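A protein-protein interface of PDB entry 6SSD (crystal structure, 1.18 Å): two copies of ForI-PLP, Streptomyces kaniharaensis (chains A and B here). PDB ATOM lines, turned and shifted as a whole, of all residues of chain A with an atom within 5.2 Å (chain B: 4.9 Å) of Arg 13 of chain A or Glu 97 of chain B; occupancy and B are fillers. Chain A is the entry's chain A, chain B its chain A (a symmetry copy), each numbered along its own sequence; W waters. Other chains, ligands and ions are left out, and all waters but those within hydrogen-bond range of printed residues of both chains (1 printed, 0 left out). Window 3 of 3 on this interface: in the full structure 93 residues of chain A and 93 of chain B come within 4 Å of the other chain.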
ATOM      1  N   ALA A   9      32.834 -24.498 -15.476  1.00  0.00           N
ATOM      2  CA  ALA A   9      32.642 -23.572 -14.365  1.00  0.00           C
ATOM      3  C   ALA A   9      31.413 -22.679 -14.573  1.00  0.00           C
ATOM      4  O   ALA A   9      30.662 -22.394 -13.631  1.00  0.00           O
ATOM      5  CB  ALA A   9      33.883 -22.718 -14.150  1.00  0.00           C
ATOM      6  N   LEU A  10      31.197 -22.229 -15.812  1.00  0.00           N
ATOM      7  CA  LEU A  10      29.986 -21.467 -16.126  1.00  0.00           C
ATOM      8  C   LEU A  10      28.747 -22.338 -15.903  1.00  0.00           C
ATOM      9  O   LEU A  10      27.754 -21.879 -15.319  1.00  0.00           O
ATOM     10  CB  LEU A  10      30.015 -20.940 -17.563  1.00  0.00           C
ATOM     11  CG  LEU A  10      30.905 -19.721 -17.735  1.00  0.00           C
ATOM     12  CD1 LEU A  10      31.253 -19.481 -19.205  1.00  0.00           C
ATOM     13  CD2 LEU A  10      30.282 -18.484 -17.121  1.00  0.00           C
ATOM     14  N   TYR A  11      28.798 -23.596 -16.334  1.00  0.00           N
ATOM     15  CA  TYR A  11      27.664 -24.497 -16.136  1.00  0.00           C
ATOM     16  C   TYR A  11      27.357 -24.703 -14.666  1.00  0.00           C
ATOM     17  O   TYR A  11      26.181 -24.754 -14.252  1.00  0.00           O
ATOM     18  CB  TYR A  11      27.911 -25.838 -16.854  1.00  0.00           C
ATOM     19  CG  TYR A  11      26.694 -26.725 -16.871  1.00  0.00           C
ATOM     20  CD1 TYR A  11      25.575 -26.331 -17.565  1.00  0.00           C
ATOM     21  CD2 TYR A  11      26.652 -27.929 -16.197  1.00  0.00           C
ATOM     22  CE1 TYR A  11      24.439 -27.101 -17.592  1.00  0.00           C
ATOM     23  CE2 TYR A  11      25.506 -28.732 -16.218  1.00  0.00           C
ATOM     24  CZ  TYR A  11      24.401 -28.301 -16.931  1.00  0.00           C
ATOM     25  OH  TYR A  11      23.236 -29.067 -16.941  1.00  0.00           O
ATOM     26  N   ALA A  12      28.389 -24.871 -13.839  1.00  0.00           N
ATOM     27  CA  ALA A  12      28.188 -25.057 -12.391  1.00  0.00           C
ATOM     28  C   ALA A  12      27.456 -23.867 -11.764  1.00  0.00           C
ATOM     29  O   ALA A  12      26.618 -24.038 -10.870  1.00  0.00           O
ATOM     30  CB  ALA A  12      29.525 -25.281 -11.686  1.00  0.00           C
ATOM     31  N   ARG A  13      27.758 -22.656 -12.214  1.00  0.00           N
ATOM     32  CA  ARG A  13      26.977 -21.506 -11.779  1.00  0.00           C
ATOM     33  C   ARG A  13      25.559 -21.523 -12.369  1.00  0.00           C
ATOM     34  O   ARG A  13      24.571 -21.238 -11.651  1.00  0.00           O
ATOM     35  CB  ARG A  13      27.688 -20.206 -12.178  1.00  0.00           C
ATOM     36  CG  ARG A  13      28.876 -19.834 -11.282  1.00  0.00           C
ATOM     37  CD  ARG A  13      29.758 -18.761 -11.891  1.00  0.00           C
ATOM     38  NE  ARG A  13      28.989 -17.546 -12.145  1.00  0.00           N
ATOM     39  CZ  ARG A  13      29.167 -16.726 -13.161  1.00  0.00           C
ATOM     40  NH1 ARG A  13      30.143 -16.927 -14.057  1.00  0.00           N
ATOM     41  NH2 ARG A  13      28.380 -15.656 -13.294  1.00  0.00           N
ATOM     42  N   ALA A  14      25.455 -21.856 -13.646  1.00  0.00           N
ATOM     43  CA  ALA A  14      24.170 -21.812 -14.337  1.00  0.00           C
ATOM     44  C   ALA A  14      23.124 -22.735 -13.740  1.00  0.00           C
ATOM     45  O   ALA A  14      21.944 -22.368 -13.655  1.00  0.00           O
ATOM     46  CB  ALA A  14      24.323 -22.105 -15.799  1.00  0.00           C
ATOM     47  N   VAL A  15      23.536 -23.927 -13.286  1.00  0.00           N
ATOM     48  CA  VAL A  15      22.539 -24.882 -12.776  1.00  0.00           C
ATOM     49  C   VAL A  15      21.872 -24.390 -11.488  1.00  0.00           C
ATOM     50  O   VAL A  15      20.811 -24.900 -11.137  1.00  0.00           O
ATOM     51  CB  VAL A  15      23.133 -26.292 -12.585  1.00  0.00           C
ATOM     52  CG1 VAL A  15      23.541 -26.897 -13.896  1.00  0.00           C
ATOM     53  CG2 VAL A  15      24.252 -26.344 -11.561  1.00  0.00           C
ATOM     54  N   GLU A  16      22.493 -23.433 -10.792  1.00  0.00           N
ATOM     55  CA  GLU A  16      21.882 -22.877  -9.584  1.00  0.00           C
ATOM     56  C   GLU A  16      20.807 -21.858  -9.867  1.00  0.00           C
ATOM     57  O   GLU A  16      19.975 -21.582  -8.984  1.00  0.00           O
ATOM     58  CB  GLU A  16      22.947 -22.264  -8.700  1.00  0.00           C
ATOM     59  CG  GLU A  16      23.988 -23.313  -8.266  1.00  0.00           C
ATOM     60  CD  GLU A  16      23.420 -24.549  -7.545  1.00  0.00           C
ATOM     61  OE1 GLU A  16      22.468 -24.419  -6.743  1.00  0.00           O
ATOM     62  OE2 GLU A  16      23.942 -25.682  -7.773  1.00  0.00           O
ATOM     63  N   VAL A  17      20.778 -21.269 -11.071  1.00  0.00           N
ATOM     64  CA  VAL A  17      19.883 -20.157 -11.396  1.00  0.00           C
ATOM     65  C   VAL A  17      19.030 -20.364 -12.632  1.00  0.00           C
ATOM     66  O   VAL A  17      18.232 -19.476 -12.954  1.00  0.00           O
ATOM     67  CB  VAL A  17      20.655 -18.817 -11.465  1.00  0.00           C
ATOM     68  CG1 VAL A  17      21.150 -18.393 -10.076  1.00  0.00           C
ATOM     69  CG2 VAL A  17      21.802 -18.867 -12.466  1.00  0.00           C
ATOM     70  N   VAL B  93      24.767 -16.234 -17.727  1.00  0.00           N
ATOM     71  CA  VAL B  93      24.916 -16.694 -16.351  1.00  0.00           C
ATOM     72  C   VAL B  93      24.971 -15.515 -15.380  1.00  0.00           C
ATOM     73  O   VAL B  93      24.312 -15.507 -14.334  1.00  0.00           O
ATOM     74  CB  VAL B  93      26.136 -17.640 -16.229  1.00  0.00           C
ATOM     75  CG1 VAL B  93      26.204 -18.217 -14.829  1.00  0.00           C
ATOM     76  CG2 VAL B  93      26.088 -18.751 -17.279  1.00  0.00           C
ATOM     77  N   GLU B  94      25.757 -14.500 -15.731  1.00  0.00           N
ATOM     78  CA  GLU B  94      25.849 -13.305 -14.919  1.00  0.00           C
ATOM     79  C   GLU B  94      24.472 -12.650 -14.729  1.00  0.00           C
ATOM     80  O   GLU B  94      24.119 -12.255 -13.610  1.00  0.00           O
ATOM     81  CB  GLU B  94      26.848 -12.328 -15.543  1.00  0.00           C
ATOM     82  CG  GLU B  94      27.028 -11.046 -14.742  1.00  0.00           C
ATOM     83  CD  GLU B  94      27.999 -10.043 -15.320  1.00  0.00           C
ATOM     84  OE1 GLU B  94      28.776 -10.389 -16.192  1.00  0.00           O
ATOM     85  OE2 GLU B  94      27.956  -8.864 -14.895  1.00  0.00           O
ATOM     86  N   TYR B  95      23.728 -12.527 -15.836  1.00  0.00           N
ATOM     87  CA  TYR B  95      22.422 -11.892 -15.763  1.00  0.00           C
ATOM     88  C   TYR B  95      21.398 -12.740 -15.020  1.00  0.00           C
ATOM     89  O   TYR B  95      20.615 -12.210 -14.231  1.00  0.00           O
ATOM     90  CB  TYR B  95      21.907 -11.507 -17.150  1.00  0.00           C
ATOM     91  CG  TYR B  95      20.612 -10.707 -17.121  1.00  0.00           C
ATOM     92  CD1 TYR B  95      20.479  -9.544 -16.394  1.00  0.00           C
ATOM     93  CD2 TYR B  95      19.506 -11.167 -17.817  1.00  0.00           C
ATOM     94  CE1 TYR B  95      19.287  -8.831 -16.376  1.00  0.00           C
ATOM     95  CE2 TYR B  95      18.338 -10.454 -17.807  1.00  0.00           C
ATOM     96  CZ  TYR B  95      18.229  -9.312 -17.085  1.00  0.00           C
ATOM     97  OH  TYR B  95      17.031  -8.608 -17.111  1.00  0.00           O
ATOM     98  N   ALA B  96      21.407 -14.066 -15.222  1.00  0.00           N
ATOM     99  CA  ALA B  96      20.487 -14.914 -14.451  1.00  0.00           C
ATOM    100  C   ALA B  96      20.745 -14.752 -12.951  1.00  0.00           C
ATOM    101  O   ALA B  96      19.797 -14.700 -12.168  1.00  0.00           O
ATOM    102  CB  ALA B  96      20.612 -16.373 -14.870  1.00  0.00           C
ATOM    103  N   GLU B  97      22.024 -14.712 -12.544  1.00  0.00           N
ATOM    104  CA  GLU B  97      22.309 -14.486 -11.126  1.00  0.00           C
ATOM    105  C   GLU B  97      21.790 -13.119 -10.663  1.00  0.00           C
ATOM    106  O   GLU B  97      21.224 -13.003  -9.571  1.00  0.00           O
ATOM    107  CB  GLU B  97      23.819 -14.567 -10.890  1.00  0.00           C
ATOM    108  CG  GLU B  97      24.397 -15.964 -11.050  1.00  0.00           C
ATOM    109  CD  GLU B  97      25.915 -16.020 -11.014  1.00  0.00           C
ATOM    110  OE1 GLU B  97      26.623 -14.973 -11.120  1.00  0.00           O
ATOM    111  OE2 GLU B  97      26.438 -17.169 -10.873  1.00  0.00           O
ATOM    112  N   ALA B  98      22.002 -12.086 -11.462  1.00  0.00           N
ATOM    113  CA  ALA B  98      21.579 -10.734 -11.090  1.00  0.00           C
ATOM    114  C   ALA B  98      20.056 -10.655 -10.926  1.00  0.00           C
ATOM    115  O   ALA B  98      19.553 -10.055  -9.975  1.00  0.00           O
ATOM    116  CB  ALA B  98      22.050  -9.732 -12.123  1.00  0.00           C
ATOM    117  N   LEU B  99      19.314 -11.247 -11.869  1.00  0.00           N
ATOM    118  CA  LEU B  99      17.845 -11.221 -11.774  1.00  0.00           C
ATOM    119  C   LEU B  99      17.332 -12.095 -10.636  1.00  0.00           C
ATOM    120  O   LEU B  99      16.453 -11.685  -9.876  1.00  0.00           O
ATOM    121  CB  LEU B  99      17.229 -11.594 -13.120  1.00  0.00           C
ATOM    122  CG  LEU B  99      15.700 -11.475 -13.168  1.00  0.00           C
ATOM    123  CD1 LEU B  99      15.220 -10.060 -12.981  1.00  0.00           C
ATOM    124  CD2 LEU B  99      15.197 -12.033 -14.517  1.00  0.00           C
ATOM    125  N   SER B 100      17.884 -13.309 -10.518  1.00  0.00           N
ATOM    126  CA  SER B 100      17.472 -14.215  -9.444  1.00  0.00           C
ATOM    127  C   SER B 100      17.636 -13.581  -8.044  1.00  0.00           C
ATOM    128  O   SER B 100      16.827 -13.796  -7.148  1.00  0.00           O
ATOM    129  CB  SER B 100      18.284 -15.534  -9.540  1.00  0.00           C
ATOM    130  OG  SER B 100      17.946 -16.411  -8.467  1.00  0.00           O
ATOM    131  N   ALA B 101      18.672 -12.752  -7.884  1.00  0.00           N
ATOM    132  CA  ALA B 101      18.960 -12.106  -6.611  1.00  0.00           C
ATOM    133  C   ALA B 101      17.880 -11.112  -6.212  1.00  0.00           C
ATOM    134  O   ALA B 101      17.858 -10.708  -5.042  1.00  0.00           O
ATOM    135  CB  ALA B 101      20.306 -11.392  -6.676  1.00  0.00           C
HETATM  136  O   HOH W   1      25.194 -19.309  -9.699  1.00  0.00           O
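OE2 of Glu 97 of chain B lies within salt-bridge range of NE of Arg 13 of chain A, at 2.9 Å.
Among the printed residues, pairs that only touch across the chains: Arg 13 of chain A with Val 93 of chain B, Val 17 of chain A with Ala 96 of chain B, Arg 13 of chain A with Glu 94 of chain B and Ala 14 of chain A with Val 93 of chain B.
Of chain B, only Val 93, Glu 94 and Glu 97 come within 4 Å of Arg 13 of chain A.
Glu 97 of chain B touches one residue of chain A.
Of the printed residues of chain A, Glu 94 of chain B touches Arg 13.
Printed residues of chain A within 4 Å of Val 93 of chain B: Arg 13 (3.6 Å) and Ala 14 (3.9 Å).
Of the printed residues of chain A, Ala 96 of chain B touches Val 17.
Printed residues of chain B within 4 Å of Val 17 of chain A: Ala 96 (3.7 Å).
Of the printed residues of chain B, Ala 14 of chain A touches Val 93 (3.9 Å).
The nearest residue of chain A that does not touch Glu 97 of chain B is Val 17 of chain A (4.1 Å).
Hydrophobic or aromatic side chains of chain A within 4 Å of the printed part of chain B: Val 17.
Printed residues of chain B that touch a printed residue of chain A: Val 93, Glu 94, Ala 96 and Glu 97.
Among the printed residues, Asp or Glu carboxylates within 4 Å of a Lys or Arg side-chain nitrogen of the other chain: Arg 13 of chain A with Glu 97 of chain B.
No position is printed for both chains.
Of the 5 pairs that touch across the chains among the printed residues, none has its exchanged pair printed and touching as well.
Water W1 bridges the side-chain carboxylate (OE2) of Glu 97 of chain B and the backbone carbonyl oxygen (O) of Arg 13 of chain A.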
